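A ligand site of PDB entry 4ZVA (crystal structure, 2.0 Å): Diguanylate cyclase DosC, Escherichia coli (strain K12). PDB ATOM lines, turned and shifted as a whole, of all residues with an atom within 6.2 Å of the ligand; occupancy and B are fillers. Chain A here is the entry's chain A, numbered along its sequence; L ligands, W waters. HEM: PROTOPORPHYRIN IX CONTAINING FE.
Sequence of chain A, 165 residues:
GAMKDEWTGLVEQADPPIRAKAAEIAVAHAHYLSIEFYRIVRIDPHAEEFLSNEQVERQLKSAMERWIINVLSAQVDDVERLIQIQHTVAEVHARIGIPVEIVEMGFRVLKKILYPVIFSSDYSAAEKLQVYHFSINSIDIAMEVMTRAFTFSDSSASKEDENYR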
ATOM      1  N   PHE A  37     -15.569 -12.335 -26.501  1.00  0.00           N
ATOM      2  CA  PHE A  37     -15.956 -11.448 -25.412  1.00  0.00           C
ATOM      3  C   PHE A  37     -14.733 -10.696 -24.881  1.00  0.00           C
ATOM      4  O   PHE A  37     -14.748  -9.473 -24.771  1.00  0.00           O
ATOM      5  CB  PHE A  37     -16.610 -12.241 -24.281  1.00  0.00           C
ATOM      6  CG  PHE A  37     -16.797 -11.475 -23.007  1.00  0.00           C
ATOM      7  CD1 PHE A  37     -17.908 -10.684 -22.801  1.00  0.00           C
ATOM      8  CD2 PHE A  37     -15.853 -11.568 -21.991  1.00  0.00           C
ATOM      9  CE1 PHE A  37     -18.085  -9.985 -21.622  1.00  0.00           C
ATOM     10  CE2 PHE A  37     -16.018 -10.870 -20.805  1.00  0.00           C
ATOM     11  CZ  PHE A  37     -17.134 -10.079 -20.621  1.00  0.00           C
ATOM     12  N   VAL A  41     -14.099  -6.624 -25.209  1.00  0.00           N
ATOM     13  CA  VAL A  41     -14.038  -5.920 -23.936  1.00  0.00           C
ATOM     14  C   VAL A  41     -12.697  -5.199 -23.757  1.00  0.00           C
ATOM     15  O   VAL A  41     -12.639  -4.073 -23.274  1.00  0.00           O
ATOM     16  CB  VAL A  41     -14.266  -6.893 -22.759  1.00  0.00           C
ATOM     17  CG1 VAL A  41     -13.712  -6.331 -21.456  1.00  0.00           C
ATOM     18  CG2 VAL A  41     -15.746  -7.227 -22.633  1.00  0.00           C
ATOM     19  N   ALA A  47     -11.956  -0.767 -19.342  1.00  0.00           N
ATOM     20  CA  ALA A  47     -12.045  -2.195 -19.024  1.00  0.00           C
ATOM     21  C   ALA A  47     -10.697  -2.879 -19.231  1.00  0.00           C
ATOM     22  O   ALA A  47     -10.416  -3.914 -18.617  1.00  0.00           O
ATOM     23  CB  ALA A  47     -13.108  -2.856 -19.873  1.00  0.00           C
ATOM     24  N   GLU A  48      -9.871  -2.312 -20.102  1.00  0.00           N
ATOM     25  CA  GLU A  48      -8.572  -2.866 -20.430  1.00  0.00           C
ATOM     26  C   GLU A  48      -7.660  -2.880 -19.202  1.00  0.00           C
ATOM     27  O   GLU A  48      -6.762  -3.711 -19.085  1.00  0.00           O
ATOM     28  CB  GLU A  48      -7.925  -2.097 -21.582  1.00  0.00           C
ATOM     29  CG  GLU A  48      -6.679  -2.731 -22.173  1.00  0.00           C
ATOM     30  CD  GLU A  48      -5.412  -2.343 -21.437  1.00  0.00           C
ATOM     31  OE1 GLU A  48      -5.426  -1.326 -20.708  1.00  0.00           O
ATOM     32  OE2 GLU A  48      -4.397  -3.063 -21.577  1.00  0.00           O
ATOM     33  N   PHE A  50      -8.358  -3.709 -16.183  1.00  0.00           N
ATOM     34  CA  PHE A  50      -8.584  -4.866 -15.336  1.00  0.00           C
ATOM     35  C   PHE A  50      -8.080  -6.154 -15.985  1.00  0.00           C
ATOM     36  O   PHE A  50      -8.100  -7.220 -15.371  1.00  0.00           O
ATOM     37  CB  PHE A  50     -10.064  -5.005 -14.996  1.00  0.00           C
ATOM     38  CG  PHE A  50     -10.650  -3.776 -14.351  1.00  0.00           C
ATOM     39  CD1 PHE A  50     -10.469  -3.537 -12.998  1.00  0.00           C
ATOM     40  CD2 PHE A  50     -11.374  -2.864 -15.094  1.00  0.00           C
ATOM     41  CE1 PHE A  50     -11.008  -2.411 -12.402  1.00  0.00           C
ATOM     42  CE2 PHE A  50     -11.917  -1.741 -14.507  1.00  0.00           C
ATOM     43  CZ  PHE A  50     -11.732  -1.515 -13.150  1.00  0.00           C
ATOM     44  N   LEU A  51      -7.634  -6.048 -17.225  1.00  0.00           N
ATOM     45  CA  LEU A  51      -7.138  -7.205 -17.967  1.00  0.00           C
ATOM     46  C   LEU A  51      -5.708  -6.936 -18.427  1.00  0.00           C
ATOM     47  O   LEU A  51      -5.465  -6.587 -19.577  1.00  0.00           O
ATOM     48  CB  LEU A  51      -8.040  -7.494 -19.168  1.00  0.00           C
ATOM     49  CG  LEU A  51      -9.549  -7.394 -18.924  1.00  0.00           C
ATOM     50  CD1 LEU A  51     -10.324  -7.544 -20.219  1.00  0.00           C
ATOM     51  CD2 LEU A  51      -9.992  -8.432 -17.898  1.00  0.00           C
ATOM     52  N   GLN A  55      -2.512 -14.406 -16.747  1.00  0.00           N
ATOM     53  CA  GLN A  55      -3.119 -15.253 -15.725  1.00  0.00           C
ATOM     54  C   GLN A  55      -4.592 -14.906 -15.528  1.00  0.00           C
ATOM     55  O   GLN A  55      -5.443 -15.791 -15.446  1.00  0.00           O
ATOM     56  CB  GLN A  55      -2.369 -15.121 -14.396  1.00  0.00           C
ATOM     57  CG  GLN A  55      -2.998 -15.847 -13.225  1.00  0.00           C
ATOM     58  CD  GLN A  55      -2.945 -17.361 -13.367  1.00  0.00           C
ATOM     59  OE1 GLN A  55      -2.178 -17.894 -14.172  1.00  0.00           O
ATOM     60  NE2 GLN A  55      -3.748 -18.062 -12.567  1.00  0.00           N
ATOM     61  N   VAL A  56      -4.893 -13.613 -15.449  1.00  0.00           N
ATOM     62  CA  VAL A  56      -6.271 -13.140 -15.347  1.00  0.00           C
ATOM     63  C   VAL A  56      -7.080 -13.467 -16.604  1.00  0.00           C
ATOM     64  O   VAL A  56      -8.200 -13.959 -16.517  1.00  0.00           O
ATOM     65  CB  VAL A  56      -6.315 -11.618 -15.093  1.00  0.00           C
ATOM     66  CG1 VAL A  56      -7.726 -11.091 -15.291  1.00  0.00           C
ATOM     67  CG2 VAL A  56      -5.799 -11.301 -13.705  1.00  0.00           C
ATOM     68  N   GLU A  57      -6.478 -13.206 -17.765  1.00  0.00           N
ATOM     69  CA  GLU A  57      -7.091 -13.485 -19.060  1.00  0.00           C
ATOM     70  C   GLU A  57      -7.517 -14.941 -19.176  1.00  0.00           C
ATOM     71  O   GLU A  57      -8.654 -15.255 -19.515  1.00  0.00           O
ATOM     72  CB  GLU A  57      -6.111 -13.158 -20.178  1.00  0.00           C
ATOM     73  CG  GLU A  57      -6.510 -13.694 -21.537  1.00  0.00           C
ATOM     74  CD  GLU A  57      -5.499 -13.357 -22.603  1.00  0.00           C
ATOM     75  OE1 GLU A  57      -4.523 -12.648 -22.303  1.00  0.00           O
ATOM     76  OE2 GLU A  57      -5.673 -13.841 -23.750  1.00  0.00           O
ATOM     77  N   GLN A  59      -7.865 -17.248 -16.748  1.00  0.00           N
ATOM     78  CA  GLN A  59      -8.875 -17.647 -15.774  1.00  0.00           C
ATOM     79  C   GLN A  59     -10.251 -17.084 -16.105  1.00  0.00           C
ATOM     80  O   GLN A  59     -11.261 -17.745 -15.899  1.00  0.00           O
ATOM     81  CB  GLN A  59      -8.464 -17.235 -14.364  1.00  0.00           C
ATOM     82  CG  GLN A  59      -7.309 -18.047 -13.781  1.00  0.00           C
ATOM     83  CD  GLN A  59      -6.987 -17.677 -12.354  1.00  0.00           C
ATOM     84  OE1 GLN A  59      -7.160 -16.531 -11.944  1.00  0.00           O
ATOM     85  NE2 GLN A  59      -6.526 -18.652 -11.580  1.00  0.00           N
ATOM     86  N   LEU A  60     -10.275 -15.853 -16.614  1.00  0.00           N
ATOM     87  CA  LEU A  60     -11.544 -15.201 -16.956  1.00  0.00           C
ATOM     88  C   LEU A  60     -12.228 -15.887 -18.123  1.00  0.00           C
ATOM     89  O   LEU A  60     -13.443 -16.076 -18.115  1.00  0.00           O
ATOM     90  CB  LEU A  60     -11.309 -13.717 -17.290  1.00  0.00           C
ATOM     91  CG  LEU A  60     -12.537 -12.914 -17.723  1.00  0.00           C
ATOM     92  CD1 LEU A  60     -13.625 -12.953 -16.657  1.00  0.00           C
ATOM     93  CD2 LEU A  60     -12.154 -11.479 -18.061  1.00  0.00           C
ATOM     94  N   ALA A  63     -13.638 -19.010 -16.849  1.00  0.00           N
ATOM     95  CA  ALA A  63     -14.775 -18.690 -15.998  1.00  0.00           C
ATOM     96  C   ALA A  63     -15.999 -18.318 -16.842  1.00  0.00           C
ATOM     97  O   ALA A  63     -17.129 -18.671 -16.497  1.00  0.00           O
ATOM     98  CB  ALA A  63     -14.416 -17.573 -15.046  1.00  0.00           C
ATOM     99  N   MET A  64     -15.772 -17.589 -17.929  1.00  0.00           N
ATOM    100  CA  MET A  64     -16.858 -17.167 -18.806  1.00  0.00           C
ATOM    101  C   MET A  64     -17.538 -18.344 -19.492  1.00  0.00           C
ATOM    102  O   MET A  64     -18.757 -18.375 -19.628  1.00  0.00           O
ATOM    103  CB  MET A  64     -16.351 -16.172 -19.857  1.00  0.00           C
ATOM    104  CG  MET A  64     -16.206 -14.737 -19.355  1.00  0.00           C
ATOM    105  SD  MET A  64     -17.782 -13.994 -18.875  1.00  0.00           S
ATOM    106  CE  MET A  64     -18.784 -14.330 -20.320  1.00  0.00           C
ATOM    107  N   ARG A  66     -17.831 -21.398 -18.389  1.00  0.00           N
ATOM    108  CA  ARG A  66     -18.646 -22.051 -17.374  1.00  0.00           C
ATOM    109  C   ARG A  66     -19.899 -21.231 -17.096  1.00  0.00           C
ATOM    110  O   ARG A  66     -20.988 -21.775 -16.952  1.00  0.00           O
ATOM    111  CB  ARG A  66     -17.839 -22.253 -16.090  1.00  0.00           C
ATOM    112  CG  ARG A  66     -18.560 -23.004 -14.994  1.00  0.00           C
ATOM    113  CD  ARG A  66     -17.721 -23.060 -13.721  1.00  0.00           C
ATOM    114  NE  ARG A  66     -16.294 -23.154 -14.024  1.00  0.00           N
ATOM    115  CZ  ARG A  66     -15.399 -22.209 -13.742  1.00  0.00           C
ATOM    116  NH1 ARG A  66     -15.785 -21.088 -13.138  1.00  0.00           N
ATOM    117  NH2 ARG A  66     -14.123 -22.376 -14.055  1.00  0.00           N
ATOM    118  N   TRP A  67     -19.739 -19.912 -17.023  1.00  0.00           N
ATOM    119  CA  TRP A  67     -20.855 -19.018 -16.741  1.00  0.00           C
ATOM    120  C   TRP A  67     -21.926 -19.120 -17.821  1.00  0.00           C
ATOM    121  O   TRP A  67     -23.115 -19.284 -17.533  1.00  0.00           O
ATOM    122  CB  TRP A  67     -20.382 -17.570 -16.609  1.00  0.00           C
ATOM    123  CG  TRP A  67     -21.439 -16.633 -16.096  1.00  0.00           C
ATOM    124  CD1 TRP A  67     -21.609 -16.217 -14.803  1.00  0.00           C
ATOM    125  CD2 TRP A  67     -22.467 -15.994 -16.860  1.00  0.00           C
ATOM    126  NE1 TRP A  67     -22.681 -15.369 -14.716  1.00  0.00           N
ATOM    127  CE2 TRP A  67     -23.221 -15.207 -15.973  1.00  0.00           C
ATOM    128  CE3 TRP A  67     -22.823 -16.001 -18.219  1.00  0.00           C
ATOM    129  CZ2 TRP A  67     -24.314 -14.444 -16.383  1.00  0.00           C
ATOM    130  CZ3 TRP A  67     -23.903 -15.239 -18.624  1.00  0.00           C
ATOM    131  CH2 TRP A  67     -24.641 -14.477 -17.708  1.00  0.00           C
ATOM    132  N   ILE A  68     -21.494 -19.009 -19.080  1.00  0.00           N
ATOM    133  CA  ILE A  68     -22.392 -19.052 -20.215  1.00  0.00           C
ATOM    134  C   ILE A  68     -23.191 -20.352 -20.247  1.00  0.00           C
ATOM    135  O   ILE A  68     -24.408 -20.338 -20.430  1.00  0.00           O
ATOM    136  CB  ILE A  68     -21.624 -18.882 -21.541  1.00  0.00           C
ATOM    137  CG1 ILE A  68     -21.058 -17.464 -21.626  1.00  0.00           C
ATOM    138  CG2 ILE A  68     -22.531 -19.162 -22.733  1.00  0.00           C
ATOM    139  CD1 ILE A  68     -20.059 -17.271 -22.741  1.00  0.00           C
ATOM    140  N   ILE A  85     -24.114 -17.969  -7.567  1.00  0.00           N
ATOM    141  CA  ILE A  85     -22.989 -17.771  -8.469  1.00  0.00           C
ATOM    142  C   ILE A  85     -22.833 -16.301  -8.853  1.00  0.00           C
ATOM    143  O   ILE A  85     -21.726 -15.762  -8.822  1.00  0.00           O
ATOM    144  CB  ILE A  85     -23.145 -18.618  -9.748  1.00  0.00           C
ATOM    145  CG1 ILE A  85     -23.043 -20.111  -9.413  1.00  0.00           C
ATOM    146  CG2 ILE A  85     -22.091 -18.240 -10.783  1.00  0.00           C
ATOM    147  CD1 ILE A  85     -23.181 -21.025 -10.610  1.00  0.00           C
ATOM    148  N   GLN A  86     -23.940 -15.659  -9.188  1.00  0.00           N
ATOM    149  CA  GLN A  86     -23.911 -14.247  -9.566  1.00  0.00           C
ATOM    150  C   GLN A  86     -23.431 -13.376  -8.415  1.00  0.00           C
ATOM    151  O   GLN A  86     -22.704 -12.409  -8.618  1.00  0.00           O
ATOM    152  CB  GLN A  86     -25.306 -13.782 -10.035  1.00  0.00           C
ATOM    153  CG  GLN A  86     -25.993 -14.719 -11.011  1.00  0.00           C
ATOM    154  CD  GLN A  86     -25.083 -15.165 -12.149  1.00  0.00           C
ATOM    155  OE1 GLN A  86     -24.332 -14.371 -12.710  1.00  0.00           O
ATOM    156  NE2 GLN A  86     -25.158 -16.445 -12.491  1.00  0.00           N
ATOM    157  N   THR A  88     -21.353 -14.363  -6.098  1.00  0.00           N
ATOM    158  CA  THR A  88     -19.921 -14.617  -6.012  1.00  0.00           C
ATOM    159  C   THR A  88     -19.149 -13.772  -7.032  1.00  0.00           C
ATOM    160  O   THR A  88     -18.126 -13.177  -6.703  1.00  0.00           O
ATOM    161  CB  THR A  88     -19.596 -16.107  -6.256  1.00  0.00           C
ATOM    162  OG1 THR A  88     -20.240 -16.910  -5.248  1.00  0.00           O
ATOM    163  CG2 THR A  88     -18.096 -16.355  -6.196  1.00  0.00           C
ATOM    164  N   VAL A  89     -19.670 -13.718  -8.249  1.00  0.00           N
ATOM    165  CA  VAL A  89     -19.044 -12.925  -9.303  1.00  0.00           C
ATOM    166  C   VAL A  89     -19.101 -11.442  -8.964  1.00  0.00           C
ATOM    167  O   VAL A  89     -18.146 -10.691  -9.220  1.00  0.00           O
ATOM    168  CB  VAL A  89     -19.739 -13.152 -10.665  1.00  0.00           C
ATOM    169  CG1 VAL A  89     -19.063 -12.340 -11.754  1.00  0.00           C
ATOM    170  CG2 VAL A  89     -19.729 -14.628 -11.021  1.00  0.00           C
ATOM    171  N   VAL A  92     -16.352 -10.662  -6.544  1.00  0.00           N
ATOM    172  CA  VAL A  92     -15.075 -10.579  -7.241  1.00  0.00           C
ATOM    173  C   VAL A  92     -14.926  -9.254  -7.979  1.00  0.00           C
ATOM    174  O   VAL A  92     -13.876  -8.603  -7.910  1.00  0.00           O
ATOM    175  CB  VAL A  92     -14.917 -11.733  -8.259  1.00  0.00           C
ATOM    176  CG1 VAL A  92     -13.604 -11.596  -9.024  1.00  0.00           C
ATOM    177  CG2 VAL A  92     -14.972 -13.070  -7.539  1.00  0.00           C
ATOM    178  N   HIS A  93     -15.973  -8.855  -8.696  1.00  0.00           N
ATOM    179  CA  HIS A  93     -15.988  -7.577  -9.414  1.00  0.00           C
ATOM    180  C   HIS A  93     -15.842  -6.405  -8.450  1.00  0.00           C
ATOM    181  O   HIS A  93     -15.185  -5.408  -8.764  1.00  0.00           O
ATOM    182  CB  HIS A  93     -17.269  -7.441 -10.228  1.00  0.00           C
ATOM    183  CG  HIS A  93     -17.307  -8.289 -11.458  1.00  0.00           C
ATOM    184  ND1 HIS A  93     -18.479  -8.555 -12.142  1.00  0.00           N
ATOM    185  CD2 HIS A  93     -16.327  -8.942 -12.123  1.00  0.00           C
ATOM    186  CE1 HIS A  93     -18.214  -9.329 -13.173  1.00  0.00           C
ATOM    187  NE2 HIS A  93     -16.923  -9.581 -13.187  1.00  0.00           N
ATOM    188  N   ILE A  96     -12.060  -6.183  -7.035  1.00  0.00           N
ATOM    189  CA  ILE A  96     -11.155  -5.665  -8.045  1.00  0.00           C
ATOM    190  C   ILE A  96     -11.403  -4.178  -8.290  1.00  0.00           C
ATOM    191  O   ILE A  96     -10.476  -3.417  -8.585  1.00  0.00           O
ATOM    192  CB  ILE A  96     -11.286  -6.448  -9.367  1.00  0.00           C
ATOM    193  CG1 ILE A  96     -11.013  -7.933  -9.124  1.00  0.00           C
ATOM    194  CG2 ILE A  96     -10.336  -5.914 -10.420  1.00  0.00           C
ATOM    195  CD1 ILE A  96     -10.968  -8.768 -10.378  1.00  0.00           C
ATOM    196  N   ILE A  98     -14.329  -2.976 -10.247  1.00  0.00           N
ATOM    197  CA  ILE A  98     -14.885  -2.825 -11.587  1.00  0.00           C
ATOM    198  C   ILE A  98     -16.240  -2.117 -11.557  1.00  0.00           C
ATOM    199  O   ILE A  98     -17.180  -2.599 -10.911  1.00  0.00           O
ATOM    200  CB  ILE A  98     -15.045  -4.186 -12.273  1.00  0.00           C
ATOM    201  CG1 ILE A  98     -13.718  -4.953 -12.237  1.00  0.00           C
ATOM    202  CG2 ILE A  98     -15.533  -4.022 -13.704  1.00  0.00           C
ATOM    203  CD1 ILE A  98     -13.813  -6.355 -12.755  1.00  0.00           C
ATOM    204  N   ILE A 102     -19.225  -0.860 -16.515  1.00  0.00           N
ATOM    205  CA  ILE A 102     -18.230  -1.657 -17.217  1.00  0.00           C
ATOM    206  C   ILE A 102     -18.713  -3.104 -17.296  1.00  0.00           C
ATOM    207  O   ILE A 102     -18.568  -3.757 -18.334  1.00  0.00           O
ATOM    208  CB  ILE A 102     -16.854  -1.590 -16.534  1.00  0.00           C
ATOM    209  CG1 ILE A 102     -16.285  -0.178 -16.643  1.00  0.00           C
ATOM    210  CG2 ILE A 102     -15.888  -2.581 -17.145  1.00  0.00           C
ATOM    211  CD1 ILE A 102     -16.070   0.270 -18.080  1.00  0.00           C
ATOM    212  N   VAL A 103     -19.296  -3.588 -16.212  1.00  0.00           N
ATOM    213  CA  VAL A 103     -19.867  -4.928 -16.185  1.00  0.00           C
ATOM    214  C   VAL A 103     -21.083  -5.019 -17.110  1.00  0.00           C
ATOM    215  O   VAL A 103     -21.219  -5.974 -17.875  1.00  0.00           O
ATOM    216  CB  VAL A 103     -20.282  -5.333 -14.749  1.00  0.00           C
ATOM    217  CG1 VAL A 103     -20.935  -6.698 -14.754  1.00  0.00           C
ATOM    218  CG2 VAL A 103     -19.086  -5.313 -13.830  1.00  0.00           C
ATOM    219  N   GLU A 104     -21.949  -4.005 -17.049  1.00  0.00           N
ATOM    220  CA  GLU A 104     -23.120  -3.944 -17.909  1.00  0.00           C
ATOM    221  C   GLU A 104     -22.721  -3.964 -19.382  1.00  0.00           C
ATOM    222  O   GLU A 104     -23.357  -4.613 -20.202  1.00  0.00           O
ATOM    223  CB  GLU A 104     -23.939  -2.686 -17.607  1.00  0.00           C
ATOM    224  CG  GLU A 104     -25.186  -2.549 -18.476  1.00  0.00           C
ATOM    225  CD  GLU A 104     -25.817  -1.178 -18.384  1.00  0.00           C
ATOM    226  OE1 GLU A 104     -26.337  -0.828 -17.305  1.00  0.00           O
ATOM    227  OE2 GLU A 104     -25.791  -0.444 -19.395  1.00  0.00           O
ATOM    228  N   MET A 105     -21.644  -3.241 -19.701  1.00  0.00           N
ATOM    229  CA  MET A 105     -21.096  -3.215 -21.054  1.00  0.00           C
ATOM    230  C   MET A 105     -20.645  -4.611 -21.479  1.00  0.00           C
ATOM    231  O   MET A 105     -20.772  -4.979 -22.654  1.00  0.00           O
ATOM    232  CB  MET A 105     -19.929  -2.231 -21.138  1.00  0.00           C
ATOM    233  CG  MET A 105     -19.290  -2.119 -22.516  1.00  0.00           C
ATOM    234  SD  MET A 105     -17.931  -3.277 -22.778  1.00  0.00           S
ATOM    235  CE  MET A 105     -16.757  -2.715 -21.538  1.00  0.00           C
ATOM    236  N   GLY A 106     -20.114  -5.373 -20.535  1.00  0.00           N
ATOM    237  CA  GLY A 106     -19.703  -6.739 -20.808  1.00  0.00           C
ATOM    238  C   GLY A 106     -20.877  -7.604 -21.214  1.00  0.00           C
ATOM    239  O   GLY A 106     -20.803  -8.382 -22.157  1.00  0.00           O
ATOM    240  N   PHE A 107     -21.986  -7.452 -20.482  1.00  0.00           N
ATOM    241  CA  PHE A 107     -23.211  -8.180 -20.790  1.00  0.00           C
ATOM    242  C   PHE A 107     -23.752  -7.827 -22.160  1.00  0.00           C
ATOM    243  O   PHE A 107     -24.291  -8.684 -22.872  1.00  0.00           O
ATOM    244  CB  PHE A 107     -24.266  -7.915 -19.725  1.00  0.00           C
ATOM    245  CG  PHE A 107     -24.112  -8.744 -18.483  1.00  0.00           C
ATOM    246  CD1 PHE A 107     -24.620 -10.031 -18.416  1.00  0.00           C
ATOM    247  CD2 PHE A 107     -23.459  -8.229 -17.380  1.00  0.00           C
ATOM    248  CE1 PHE A 107     -24.485 -10.790 -17.270  1.00  0.00           C
ATOM    249  CE2 PHE A 107     -23.311  -8.989 -16.228  1.00  0.00           C
ATOM    250  CZ  PHE A 107     -23.824 -10.276 -16.182  1.00  0.00           C
ATOM    251  N   LEU A 110     -21.651  -9.570 -24.758  1.00  0.00           N
ATOM    252  CA  LEU A 110     -21.996 -10.991 -24.774  1.00  0.00           C
ATOM    253  C   LEU A 110     -23.286 -11.235 -25.554  1.00  0.00           C
ATOM    254  O   LEU A 110     -23.332 -12.108 -26.427  1.00  0.00           O
ATOM    255  CB  LEU A 110     -22.152 -11.517 -23.343  1.00  0.00           C
ATOM    256  CG  LEU A 110     -22.567 -12.996 -23.222  1.00  0.00           C
ATOM    257  CD1 LEU A 110     -21.533 -13.904 -23.894  1.00  0.00           C
ATOM    258  CD2 LEU A 110     -22.778 -13.382 -21.767  1.00  0.00           C
ATOM    259  N   ILE A 139     -29.843 -14.143 -19.757  1.00  0.00           N
ATOM    260  CA  ILE A 139     -28.652 -13.343 -19.512  1.00  0.00           C
ATOM    261  C   ILE A 139     -29.024 -12.086 -18.735  1.00  0.00           C
ATOM    262  O   ILE A 139     -28.310 -11.677 -17.809  1.00  0.00           O
ATOM    263  CB  ILE A 139     -27.954 -12.965 -20.838  1.00  0.00           C
ATOM    264  CG1 ILE A 139     -27.375 -14.222 -21.491  1.00  0.00           C
ATOM    265  CG2 ILE A 139     -26.833 -11.958 -20.593  1.00  0.00           C
ATOM    266  CD1 ILE A 139     -26.682 -13.967 -22.793  1.00  0.00           C
ATOM    267  N   MET A 146     -26.629 -10.052 -10.424  1.00  0.00           N
ATOM    268  CA  MET A 146     -25.240  -9.651 -10.219  1.00  0.00           C
ATOM    269  C   MET A 146     -25.118  -8.174  -9.859  1.00  0.00           C
ATOM    270  O   MET A 146     -24.365  -7.809  -8.956  1.00  0.00           O
ATOM    271  CB  MET A 146     -24.405  -9.952 -11.471  1.00  0.00           C
ATOM    272  CG  MET A 146     -22.917  -9.719 -11.287  1.00  0.00           C
ATOM    273  SD  MET A 146     -21.984  -9.982 -12.802  1.00  0.00           S
ATOM    274  CE  MET A 146     -22.403 -11.691 -13.157  1.00  0.00           C
HETATM  275  CHA HEM L   1     -14.077 -12.528 -12.740  1.00  0.00           C
HETATM  276  CHB HEM L   1     -13.253  -8.510 -15.343  1.00  0.00           C
HETATM  277  CHC HEM L   1     -17.802  -8.724 -16.963  1.00  0.00           C
HETATM  278  CHD HEM L   1     -18.223 -13.237 -15.251  1.00  0.00           C
HETATM  279  C1A HEM L   1     -13.436 -11.446 -13.316  1.00  0.00           C
HETATM  280  C2A HEM L   1     -12.035 -11.079 -13.174  1.00  0.00           C
HETATM  281  C3A HEM L   1     -11.822  -9.981 -13.890  1.00  0.00           C
HETATM  282  C4A HEM L   1     -13.068  -9.596 -14.521  1.00  0.00           C
HETATM  283  CMA HEM L   1     -10.484  -9.226 -14.041  1.00  0.00           C
HETATM  284  CAA HEM L   1     -10.967 -11.819 -12.348  1.00  0.00           C
HETATM  285  CBA HEM L   1     -10.817 -13.251 -12.856  1.00  0.00           C
HETATM  286  CGA HEM L   1      -9.582 -13.881 -12.276  1.00  0.00           C
HETATM  287  O1A HEM L   1      -8.613 -13.143 -11.974  1.00  0.00           O
HETATM  288  O2A HEM L   1      -9.575 -15.134 -12.113  1.00  0.00           O
HETATM  289  C1B HEM L   1     -14.408  -8.228 -16.034  1.00  0.00           C
HETATM  290  C2B HEM L   1     -14.583  -7.164 -16.996  1.00  0.00           C
HETATM  291  C3B HEM L   1     -15.853  -7.214 -17.438  1.00  0.00           C
HETATM  292  C4B HEM L   1     -16.503  -8.327 -16.782  1.00  0.00           C
HETATM  293  CMB HEM L   1     -13.457  -6.167 -17.369  1.00  0.00           C
HETATM  294  CAB HEM L   1     -16.596  -6.327 -18.476  1.00  0.00           C
HETATM  295  CBB HEM L   1     -16.032  -5.346 -19.172  1.00  0.00           C
HETATM  296  C1C HEM L   1     -18.289  -9.991 -16.721  1.00  0.00           C
HETATM  297  C2C HEM L   1     -19.503 -10.571 -17.275  1.00  0.00           C
HETATM  298  C3C HEM L   1     -19.623 -11.815 -16.795  1.00  0.00           C
HETATM  299  C4C HEM L   1     -18.477 -12.066 -15.931  1.00  0.00           C
HETATM  300  CMC HEM L   1     -20.441  -9.794 -18.234  1.00  0.00           C
HETATM  301  CAC HEM L   1     -20.711 -12.882 -17.054  1.00  0.00           C
HETATM  302  CBC HEM L   1     -21.737 -12.736 -17.907  1.00  0.00           C
HETATM  303  C1D HEM L   1     -17.161 -13.481 -14.408  1.00  0.00           C
HETATM  304  C2D HEM L   1     -16.937 -14.707 -13.676  1.00  0.00           C
HETATM  305  C3D HEM L   1     -15.637 -14.488 -12.890  1.00  0.00           C
HETATM  306  C4D HEM L   1     -15.209 -13.143 -13.222  1.00  0.00           C
HETATM  307  CMD HEM L   1     -17.838 -15.961 -13.702  1.00  0.00           C
HETATM  308  CAD HEM L   1     -14.928 -15.463 -11.928  1.00  0.00           C
HETATM  309  CBD HEM L   1     -15.839 -15.795 -10.757  1.00  0.00           C
HETATM  310  CGD HEM L   1     -15.053 -16.398  -9.630  1.00  0.00           C
HETATM  311  O1D HEM L   1     -15.675 -16.966  -8.693  1.00  0.00           O
HETATM  312  O2D HEM L   1     -13.793 -16.327  -9.655  1.00  0.00           O
HETATM  313  NA  HEM L   1     -14.032 -10.517 -14.145  1.00  0.00           N
HETATM  314  NB  HEM L   1     -15.596  -8.931 -15.923  1.00  0.00           N
HETATM  315  NC  HEM L   1     -17.694 -10.933 -15.910  1.00  0.00           N
HETATM  316  ND  HEM L   1     -16.127 -12.585 -14.115  1.00  0.00           N
HETATM  317 FE   HEM L   1     -15.978 -10.633 -14.828  1.00  0.00          FE
HETATM  318  O   HOH W   1     -15.129 -19.466  -8.096  1.00  0.00           O
HETATM  319  O   HOH W   2     -18.230 -19.367 -13.978  1.00  0.00           O
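NE2 of His 93 binds FE of the ligand (2.2 Å). OE1 of Gln 59 lies close to O2A of the ligand (2.8 Å).
O of His 93 lies within hydrogen-bond range of N of Ile 98 (3.0 Å). The side-chain amide nitrogen of Gln 55 sits close to the side-chain amide nitrogen of Gln 59, at 3.0 Å. NE1 of Trp 67 is in hydrogen-bond range of OE1 of Gln 86, at 2.8 Å.
Phe 37 touches the ligand. Val 41 touches the ligand. CB of Ala 47 touches CBB of the ligand, 3.9 Å away. Phe 50 touches the ligand (O to CMA, 3.4 Å). Leu 51 touches the ligand. Val 56 touches the ligand (CG1 to CMA, 3.6 Å). Leu 60 touches the ligand (CD1 to NA, 3.5 Å). Ala 63 touches the ligand (CB to CAD, 3.8 Å). Met 64 touches the ligand. Trp 67 touches the ligand. Thr 88 touches the ligand (CG2 to O1D, 3.5 Å). CG1 of Val 89 touches C1D of the ligand, 3.5 Å away. Val 92 touches the ligand. Ile 96 touches the ligand. Ile 98 touches the ligand (CD1 to CHB, 3.4 Å). Ile 102 touches the ligand (O to CBB, 3.1 Å). Val 103 touches the ligand (O to CMC, 3.9 Å). Met 105 touches the ligand. Gly 106 touches the ligand. Phe 107 touches the ligand. Of the 33 residues printed, 22 come within 4 Å of the ligand. Along chain A the residues within 4 Å of the ligand span positions 37 to 107. The nearest printed residue that does not touch the ligand is Leu 110 (4.05 Å).
Water W2 lies within hydrogen-bond range of O of Ala 63, NH1 of Arg 66 and N of Trp 67.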
